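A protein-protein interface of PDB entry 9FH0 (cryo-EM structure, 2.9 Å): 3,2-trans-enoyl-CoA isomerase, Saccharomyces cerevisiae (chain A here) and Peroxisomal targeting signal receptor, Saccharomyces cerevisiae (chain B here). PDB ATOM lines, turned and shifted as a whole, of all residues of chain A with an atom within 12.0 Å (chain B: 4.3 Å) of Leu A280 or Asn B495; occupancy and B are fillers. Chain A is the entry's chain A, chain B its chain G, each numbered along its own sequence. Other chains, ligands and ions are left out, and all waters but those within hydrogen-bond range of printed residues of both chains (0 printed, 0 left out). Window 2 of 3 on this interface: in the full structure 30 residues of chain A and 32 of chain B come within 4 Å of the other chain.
O of Asn B393 is in hydrogen-bond range of N of Arg A276 (3.3 Å).
N of Arg A279 sits at hydrogen-bond distance from OD1 of Asn B530 (3.0 Å).
The backbone NH (N) of Leu A280 lies close to the side-chain amide nitrogen (ND2) of Asn B393 (2.9 Å).
The backbone carbonyl oxygen (O) of Arg A276 lies within hydrogen-bond range of the guanidinium group (NH1) of Arg A279 (3.3 Å).
The side-chain amide oxygen (OD1) of Asn B393 lies within hydrogen-bond range of the guanidinium group (NH1) of Arg B526, at 2.8 Å.
NH2 of Arg B496 lies within hydrogen-bond range of SD of Met B493.
The side-chain amide oxygen of Asn B495 is in hydrogen-bond range of the side-chain amide nitrogen of Asn B530 (3.2 Å).
N of Ala B499 sits at hydrogen-bond distance from OH of Tyr B514 (3.3 Å).
ND2 of Asn B530 is in hydrogen-bond range of O of Arg B526 (3.1 Å).
CD of Arg A276 touches CE1 of Tyr B468, 3.9 Å away.
CA of His A278 touches OD1 of Asn B530, at 3.5 Å.
Asn B393 touches Arg A279.
CB of Ala B499 touches O of Arg A279, 3.0 Å away.
Arg A279 touches Arg B526 (CB to NH1, 3.2 Å).
CD2 of Leu A280 touches ND2 of Asn B495, at 3.2 Å.
CD2 of Leu A280 touches NE of Arg B496 (3.4 Å).
Leu A280 touches Ala B499 (C to CB, 3.8 Å).
Leu A280 touches Arg B526.
Of the printed residues of chain B, His A278 touches Asn B530.
Of the printed residues of chain B, Arg A279 touches Asn B393, Ala B499, Arg B526 and Asn B530.
Of the printed residues of chain B, Leu A280 touches Asn B393, Asn B495, Arg B496, Ala B499 and Arg B526.
Printed residues of chain A within 4 Å of Asn B393: Arg A276, Arg A279 and Leu A280.
No residue of chain A comes within 4 Å of Met B493.
Asn B495 touches one residue of chain A.
Arg B496 touches one residue of chain A.
Leu B497 touches none of the printed residues of chain A.
No residue of chain A comes within 4 Å of Gly B498.
Of chain A, only Arg A279 (3.0 Å) and Leu A280 (3.8 Å) come within 4 Å of Ala B499.
Tyr B514 touches none of the printed residues of chain A.
Of chain A, only Arg A279 (3.2 Å) and Leu A280 (3.0 Å) come within 4 Å of Arg B526.
Of chain A, only His A278 (3.5 Å) and Arg A279 (3.0 Å) come within 4 Å of Asn B530.
The nearest printed residue of chain B that does not touch Leu A280 is Ile B389 (4.01 Å).
The nearest residue of chain A that does not touch Asn B495 is Arg A279 (4.05 Å).
Printed residues of chain B that touch a printed residue of chain A: Asn B393, Tyr B468, Asn B495, Arg B496, Ala B499, Arg B526 and Asn B530.
Of the 7 printed residues of chain A, 4 touch a printed residue of chain B.
Hydrophobic or aromatic side chains of chain A that line the printed part of chain B: His A278 and Leu A280.
Among the printed residues, no Asp or Glu carboxylate lies within 4 Å of a Lys or Arg side-chain nitrogen of the other chain.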
ATOM      1  N   LYS A 274       1.810 -11.679  10.360  1.00  0.00           N
ATOM      2  CA  LYS A 274       0.526 -11.046  10.098  1.00  0.00           C
ATOM      3  C   LYS A 274      -0.205 -10.653  11.374  1.00  0.00           C
ATOM      4  O   LYS A 274      -1.422 -10.788  11.462  1.00  0.00           O
ATOM      5  CB  LYS A 274      -0.363 -11.965   9.269  1.00  0.00           C
ATOM      6  CG  LYS A 274       0.229 -12.405   7.957  1.00  0.00           C
ATOM      7  CD  LYS A 274       0.754 -11.227   7.180  1.00  0.00           C
ATOM      8  CE  LYS A 274       1.123 -11.619   5.770  1.00  0.00           C
ATOM      9  NZ  LYS A 274      -0.078 -11.948   4.965  1.00  0.00           N
ATOM     10  N   GLN A 275       0.513 -10.157  12.373  1.00  0.00           N
ATOM     11  CA  GLN A 275      -0.145  -9.737  13.601  1.00  0.00           C
ATOM     12  C   GLN A 275      -1.147  -8.635  13.305  1.00  0.00           C
ATOM     13  O   GLN A 275      -0.960  -7.827  12.397  1.00  0.00           O
ATOM     14  CB  GLN A 275       0.874  -9.250  14.623  1.00  0.00           C
ATOM     15  CG  GLN A 275       1.755 -10.331  15.167  1.00  0.00           C
ATOM     16  CD  GLN A 275       2.921 -10.628  14.256  1.00  0.00           C
ATOM     17  OE1 GLN A 275       3.294  -9.800  13.432  1.00  0.00           O
ATOM     18  NE2 GLN A 275       3.500 -11.819  14.389  1.00  0.00           N
ATOM     19  N   ARG A 276      -2.222  -8.610  14.073  1.00  0.00           N
ATOM     20  CA  ARG A 276      -3.291  -7.660  13.836  1.00  0.00           C
ATOM     21  C   ARG A 276      -3.064  -6.381  14.632  1.00  0.00           C
ATOM     22  O   ARG A 276      -2.264  -6.335  15.567  1.00  0.00           O
ATOM     23  CB  ARG A 276      -4.636  -8.283  14.176  1.00  0.00           C
ATOM     24  CG  ARG A 276      -5.121  -9.215  13.106  1.00  0.00           C
ATOM     25  CD  ARG A 276      -6.557  -9.604  13.317  1.00  0.00           C
ATOM     26  NE  ARG A 276      -7.160 -10.115  12.096  1.00  0.00           N
ATOM     27  CZ  ARG A 276      -7.209 -11.396  11.768  1.00  0.00           C
ATOM     28  NH1 ARG A 276      -7.771 -11.767  10.637  1.00  0.00           N
ATOM     29  NH2 ARG A 276      -6.700 -12.305  12.570  1.00  0.00           N
ATOM     30  N   LYS A 277      -3.775  -5.325  14.234  1.00  0.00           N
ATOM     31  CA  LYS A 277      -3.530  -4.005  14.804  1.00  0.00           C
ATOM     32  C   LYS A 277      -4.119  -3.882  16.202  1.00  0.00           C
ATOM     33  O   LYS A 277      -3.408  -3.571  17.161  1.00  0.00           O
ATOM     34  CB  LYS A 277      -4.099  -2.927  13.883  1.00  0.00           C
ATOM     35  N   HIS A 278      -5.415  -4.112  16.333  1.00  0.00           N
ATOM     36  CA  HIS A 278      -6.100  -4.104  17.613  1.00  0.00           C
ATOM     37  C   HIS A 278      -6.253  -5.527  18.132  1.00  0.00           C
ATOM     38  O   HIS A 278      -6.065  -6.503  17.406  1.00  0.00           O
ATOM     39  CB  HIS A 278      -7.461  -3.435  17.474  1.00  0.00           C
ATOM     40  CG  HIS A 278      -7.457  -2.270  16.538  1.00  0.00           C
ATOM     41  ND1 HIS A 278      -7.006  -1.024  16.905  1.00  0.00           N
ATOM     42  CD2 HIS A 278      -7.831  -2.169  15.242  1.00  0.00           C
ATOM     43  CE1 HIS A 278      -7.111  -0.202  15.877  1.00  0.00           C
ATOM     44  NE2 HIS A 278      -7.610  -0.873  14.856  1.00  0.00           N
ATOM     45  N   ARG A 279      -6.598  -5.640  19.405  1.00  0.00           N
ATOM     46  CA  ARG A 279      -6.532  -6.914  20.098  1.00  0.00           C
ATOM     47  C   ARG A 279      -7.912  -7.389  20.530  1.00  0.00           C
ATOM     48  O   ARG A 279      -8.757  -6.595  20.937  1.00  0.00           O
ATOM     49  CB  ARG A 279      -5.621  -6.799  21.309  1.00  0.00           C
ATOM     50  CG  ARG A 279      -4.257  -6.277  20.988  1.00  0.00           C
ATOM     51  CD  ARG A 279      -3.512  -7.313  20.228  1.00  0.00           C
ATOM     52  NE  ARG A 279      -2.350  -6.769  19.552  1.00  0.00           N
ATOM     53  CZ  ARG A 279      -1.482  -7.514  18.886  1.00  0.00           C
ATOM     54  NH1 ARG A 279      -0.444  -6.955  18.286  1.00  0.00           N
ATOM     55  NH2 ARG A 279      -1.653  -8.822  18.828  1.00  0.00           N
ATOM     56  N   LEU A 280      -8.104  -8.702  20.475  1.00  0.00           N
ATOM     57  CA  LEU A 280      -9.386  -9.356  20.736  1.00  0.00           C
ATOM     58  C   LEU A 280     -10.445  -8.995  19.706  1.00  0.00           C
ATOM     59  O   LEU A 280     -10.852  -9.843  18.917  1.00  0.00           O
ATOM     60  CB  LEU A 280      -9.884  -9.042  22.148  1.00  0.00           C
ATOM     61  CG  LEU A 280      -9.526 -10.037  23.255  1.00  0.00           C
ATOM     62  CD1 LEU A 280      -8.071 -10.047  23.565  1.00  0.00           C
ATOM     63  CD2 LEU A 280     -10.307  -9.745  24.529  1.00  0.00           C
ATOM     64  N   ILE B 389      -8.808 -17.198  20.541  1.00  0.00           N
ATOM     65  CA  ILE B 389      -8.795 -15.741  20.444  1.00  0.00           C
ATOM     66  C   ILE B 389      -7.375 -15.216  20.292  1.00  0.00           C
ATOM     67  O   ILE B 389      -7.117 -14.307  19.499  1.00  0.00           O
ATOM     68  CB  ILE B 389      -9.490 -15.115  21.654  1.00  0.00           C
ATOM     69  CG1 ILE B 389     -10.894 -15.667  21.790  1.00  0.00           C
ATOM     70  CG2 ILE B 389      -9.548 -13.635  21.494  1.00  0.00           C
ATOM     71  CD1 ILE B 389     -11.607 -15.145  22.977  1.00  0.00           C
ATOM     72  N   ASN B 393      -5.587 -13.128  17.255  1.00  0.00           N
ATOM     73  CA  ASN B 393      -4.827 -11.899  17.459  1.00  0.00           C
ATOM     74  C   ASN B 393      -3.492 -11.941  16.742  1.00  0.00           C
ATOM     75  O   ASN B 393      -3.043 -10.929  16.201  1.00  0.00           O
ATOM     76  CB  ASN B 393      -4.599 -11.654  18.941  1.00  0.00           C
ATOM     77  CG  ASN B 393      -5.766 -11.011  19.592  1.00  0.00           C
ATOM     78  OD1 ASN B 393      -5.856 -10.951  20.809  1.00  0.00           O
ATOM     79  ND2 ASN B 393      -6.684 -10.520  18.781  1.00  0.00           N
ATOM     80  N   TYR B 468     -15.265 -11.958  12.246  1.00  0.00           N
ATOM     81  CA  TYR B 468     -14.177 -11.011  12.435  1.00  0.00           C
ATOM     82  C   TYR B 468     -13.006 -11.342  11.531  1.00  0.00           C
ATOM     83  O   TYR B 468     -12.457 -10.465  10.863  1.00  0.00           O
ATOM     84  CB  TYR B 468     -13.755 -11.019  13.900  1.00  0.00           C
ATOM     85  CG  TYR B 468     -12.612 -10.108  14.260  1.00  0.00           C
ATOM     86  CD1 TYR B 468     -11.305 -10.507  14.088  1.00  0.00           C
ATOM     87  CD2 TYR B 468     -12.845  -8.868  14.810  1.00  0.00           C
ATOM     88  CE1 TYR B 468     -10.272  -9.690  14.424  1.00  0.00           C
ATOM     89  CE2 TYR B 468     -11.820  -8.047  15.150  1.00  0.00           C
ATOM     90  CZ  TYR B 468     -10.535  -8.459  14.959  1.00  0.00           C
ATOM     91  OH  TYR B 468      -9.497  -7.630  15.302  1.00  0.00           O
ATOM     92  N   GLU B 491     -16.136  -7.449  30.881  1.00  0.00           N
ATOM     93  CA  GLU B 491     -15.084  -6.557  30.412  1.00  0.00           C
ATOM     94  C   GLU B 491     -14.475  -7.039  29.108  1.00  0.00           C
ATOM     95  O   GLU B 491     -14.184  -6.226  28.224  1.00  0.00           O
ATOM     96  CB  GLU B 491     -13.993  -6.392  31.476  1.00  0.00           C
ATOM     97  CG  GLU B 491     -13.333  -7.658  31.942  1.00  0.00           C
ATOM     98  CD  GLU B 491     -14.127  -8.363  33.017  1.00  0.00           C
ATOM     99  OE1 GLU B 491     -15.362  -8.196  33.060  1.00  0.00           O
ATOM    100  OE2 GLU B 491     -13.513  -9.085  33.827  1.00  0.00           O
ATOM    101  N   LEU B 492     -14.290  -8.345  28.960  1.00  0.00           N
ATOM    102  CA  LEU B 492     -13.697  -8.854  27.735  1.00  0.00           C
ATOM    103  C   LEU B 492     -14.606  -8.610  26.544  1.00  0.00           C
ATOM    104  O   LEU B 492     -14.125  -8.342  25.445  1.00  0.00           O
ATOM    105  CB  LEU B 492     -13.392 -10.332  27.879  1.00  0.00           C
ATOM    106  CG  LEU B 492     -12.747 -10.686  29.203  1.00  0.00           C
ATOM    107  CD1 LEU B 492     -12.500 -12.170  29.268  1.00  0.00           C
ATOM    108  CD2 LEU B 492     -11.466  -9.928  29.348  1.00  0.00           C
ATOM    109  N   MET B 493     -15.918  -8.700  26.733  1.00  0.00           N
ATOM    110  CA  MET B 493     -16.821  -8.444  25.620  1.00  0.00           C
ATOM    111  C   MET B 493     -16.826  -6.976  25.234  1.00  0.00           C
ATOM    112  O   MET B 493     -16.926  -6.649  24.049  1.00  0.00           O
ATOM    113  CB  MET B 493     -18.225  -8.910  25.964  1.00  0.00           C
ATOM    114  CG  MET B 493     -18.379 -10.397  25.870  1.00  0.00           C
ATOM    115  SD  MET B 493     -17.859 -11.002  24.262  1.00  0.00           S
ATOM    116  CE  MET B 493     -19.011 -10.133  23.221  1.00  0.00           C
ATOM    117  N   TRP B 494     -16.695  -6.079  26.204  1.00  0.00           N
ATOM    118  CA  TRP B 494     -16.579  -4.670  25.869  1.00  0.00           C
ATOM    119  C   TRP B 494     -15.274  -4.391  25.143  1.00  0.00           C
ATOM    120  O   TRP B 494     -15.245  -3.604  24.196  1.00  0.00           O
ATOM    121  CB  TRP B 494     -16.701  -3.830  27.128  1.00  0.00           C
ATOM    122  CG  TRP B 494     -18.110  -3.547  27.477  1.00  0.00           C
ATOM    123  CD1 TRP B 494     -18.796  -4.044  28.524  1.00  0.00           C
ATOM    124  CD2 TRP B 494     -19.016  -2.707  26.767  1.00  0.00           C
ATOM    125  NE1 TRP B 494     -20.075  -3.568  28.524  1.00  0.00           N
ATOM    126  CE2 TRP B 494     -20.234  -2.742  27.448  1.00  0.00           C
ATOM    127  CE3 TRP B 494     -18.911  -1.924  25.616  1.00  0.00           C
ATOM    128  CZ2 TRP B 494     -21.340  -2.031  27.025  1.00  0.00           C
ATOM    129  CZ3 TRP B 494     -20.013  -1.218  25.197  1.00  0.00           C
ATOM    130  CH2 TRP B 494     -21.209  -1.274  25.896  1.00  0.00           C
ATOM    131  N   ASN B 495     -14.191  -5.058  25.535  1.00  0.00           N
ATOM    132  CA  ASN B 495     -12.933  -4.879  24.820  1.00  0.00           C
ATOM    133  C   ASN B 495     -12.968  -5.485  23.421  1.00  0.00           C
ATOM    134  O   ASN B 495     -12.379  -4.927  22.492  1.00  0.00           O
ATOM    135  CB  ASN B 495     -11.788  -5.481  25.606  1.00  0.00           C
ATOM    136  CG  ASN B 495     -10.514  -5.493  24.825  1.00  0.00           C
ATOM    137  OD1 ASN B 495     -10.203  -4.549  24.117  1.00  0.00           O
ATOM    138  ND2 ASN B 495      -9.765  -6.568  24.943  1.00  0.00           N
ATOM    139  N   ARG B 496     -13.644  -6.617  23.242  1.00  0.00           N
ATOM    140  CA  ARG B 496     -13.787  -7.176  21.906  1.00  0.00           C
ATOM    141  C   ARG B 496     -14.672  -6.305  21.036  1.00  0.00           C
ATOM    142  O   ARG B 496     -14.443  -6.195  19.829  1.00  0.00           O
ATOM    143  CB  ARG B 496     -14.343  -8.586  21.989  1.00  0.00           C
ATOM    144  CG  ARG B 496     -13.334  -9.570  22.489  1.00  0.00           C
ATOM    145  CD  ARG B 496     -13.963 -10.842  22.946  1.00  0.00           C
ATOM    146  NE  ARG B 496     -13.077 -11.555  23.844  1.00  0.00           N
ATOM    147  CZ  ARG B 496     -13.487 -12.454  24.722  1.00  0.00           C
ATOM    148  NH1 ARG B 496     -12.612 -13.059  25.505  1.00  0.00           N
ATOM    149  NH2 ARG B 496     -14.772 -12.747  24.814  1.00  0.00           N
ATOM    150  N   LEU B 497     -15.673  -5.668  21.627  1.00  0.00           N
ATOM    151  CA  LEU B 497     -16.455  -4.697  20.883  1.00  0.00           C
ATOM    152  C   LEU B 497     -15.597  -3.509  20.482  1.00  0.00           C
ATOM    153  O   LEU B 497     -15.683  -3.027  19.349  1.00  0.00           O
ATOM    154  CB  LEU B 497     -17.648  -4.262  21.722  1.00  0.00           C
ATOM    155  CG  LEU B 497     -18.652  -3.295  21.113  1.00  0.00           C
ATOM    156  CD1 LEU B 497     -19.143  -3.792  19.776  1.00  0.00           C
ATOM    157  CD2 LEU B 497     -19.798  -3.131  22.073  1.00  0.00           C
ATOM    158  N   GLY B 498     -14.746  -3.040  21.389  1.00  0.00           N
ATOM    159  CA  GLY B 498     -13.840  -1.960  21.044  1.00  0.00           C
ATOM    160  C   GLY B 498     -12.919  -2.313  19.892  1.00  0.00           C
ATOM    161  O   GLY B 498     -12.708  -1.510  18.984  1.00  0.00           O
ATOM    162  N   ALA B 499     -12.372  -3.526  19.905  1.00  0.00           N
ATOM    163  CA  ALA B 499     -11.492  -3.937  18.817  1.00  0.00           C
ATOM    164  C   ALA B 499     -12.248  -4.085  17.504  1.00  0.00           C
ATOM    165  O   ALA B 499     -11.763  -3.657  16.450  1.00  0.00           O
ATOM    166  CB  ALA B 499     -10.796  -5.240  19.163  1.00  0.00           C
ATOM    167  N   TYR B 514     -13.660   0.954  25.094  1.00  0.00           N
ATOM    168  CA  TYR B 514     -12.473   0.769  25.919  1.00  0.00           C
ATOM    169  C   TYR B 514     -12.640   1.431  27.277  1.00  0.00           C
ATOM    170  O   TYR B 514     -12.233   0.874  28.303  1.00  0.00           O
ATOM    171  CB  TYR B 514     -11.248   1.333  25.215  1.00  0.00           C
ATOM    172  CG  TYR B 514     -10.917   0.638  23.934  1.00  0.00           C
ATOM    173  CD1 TYR B 514     -11.145  -0.707  23.779  1.00  0.00           C
ATOM    174  CD2 TYR B 514     -10.377   1.332  22.881  1.00  0.00           C
ATOM    175  CE1 TYR B 514     -10.836  -1.338  22.614  1.00  0.00           C
ATOM    176  CE2 TYR B 514     -10.070   0.710  21.712  1.00  0.00           C
ATOM    177  CZ  TYR B 514     -10.303  -0.622  21.580  1.00  0.00           C
ATOM    178  OH  TYR B 514      -9.985  -1.239  20.398  1.00  0.00           O
ATOM    179  N   ALA B 517     -14.855  -0.911  29.326  1.00  0.00           N
ATOM    180  CA  ALA B 517     -14.094  -2.048  29.826  1.00  0.00           C
ATOM    181  C   ALA B 517     -13.229  -1.640  31.004  1.00  0.00           C
ATOM    182  O   ALA B 517     -13.158  -2.344  32.014  1.00  0.00           O
ATOM    183  CB  ALA B 517     -13.230  -2.635  28.714  1.00  0.00           C
ATOM    184  N   PHE B 524      -7.093  -3.942  33.639  1.00  0.00           N
ATOM    185  CA  PHE B 524      -7.135  -4.555  32.315  1.00  0.00           C
ATOM    186  C   PHE B 524      -6.213  -3.775  31.388  1.00  0.00           C
ATOM    187  O   PHE B 524      -6.561  -2.696  30.916  1.00  0.00           O
ATOM    188  CB  PHE B 524      -8.575  -4.579  31.826  1.00  0.00           C
ATOM    189  CG  PHE B 524      -8.822  -5.484  30.673  1.00  0.00           C
ATOM    190  CD1 PHE B 524      -8.269  -6.728  30.618  1.00  0.00           C
ATOM    191  CD2 PHE B 524      -9.678  -5.111  29.673  1.00  0.00           C
ATOM    192  CE1 PHE B 524      -8.523  -7.552  29.558  1.00  0.00           C
ATOM    193  CE2 PHE B 524      -9.928  -5.940  28.621  1.00  0.00           C
ATOM    194  CZ  PHE B 524      -9.351  -7.154  28.566  1.00  0.00           C
ATOM    195  N   ARG B 526      -4.827  -4.846  28.428  1.00  0.00           N
ATOM    196  CA  ARG B 526      -5.247  -5.004  27.041  1.00  0.00           C
ATOM    197  C   ARG B 526      -6.075  -3.811  26.578  1.00  0.00           C
ATOM    198  O   ARG B 526      -5.843  -3.248  25.499  1.00  0.00           O
ATOM    199  CB  ARG B 526      -6.031  -6.315  26.930  1.00  0.00           C
ATOM    200  CG  ARG B 526      -6.630  -6.654  25.597  1.00  0.00           C
ATOM    201  CD  ARG B 526      -5.585  -7.129  24.658  1.00  0.00           C
ATOM    202  NE  ARG B 526      -4.925  -8.341  25.104  1.00  0.00           N
ATOM    203  CZ  ARG B 526      -4.732  -9.414  24.350  1.00  0.00           C
ATOM    204  NH1 ARG B 526      -5.124  -9.430  23.095  1.00  0.00           N
ATOM    205  NH2 ARG B 526      -4.113 -10.465  24.847  1.00  0.00           N
ATOM    206  N   ASN B 530      -5.238  -0.891  23.691  1.00  0.00           N
ATOM    207  CA  ASN B 530      -6.114  -0.619  22.552  1.00  0.00           C
ATOM    208  C   ASN B 530      -6.574   0.834  22.549  1.00  0.00           C
ATOM    209  O   ASN B 530      -6.632   1.483  21.492  1.00  0.00           O
ATOM    210  CB  ASN B 530      -7.318  -1.556  22.589  1.00  0.00           C
ATOM    211  CG  ASN B 530      -7.003  -2.935  22.066  1.00  0.00           C
ATOM    212  OD1 ASN B 530      -6.449  -3.087  20.987  1.00  0.00           O
ATOM    213  ND2 ASN B 530      -7.360  -3.949  22.831  1.00  0.00           N
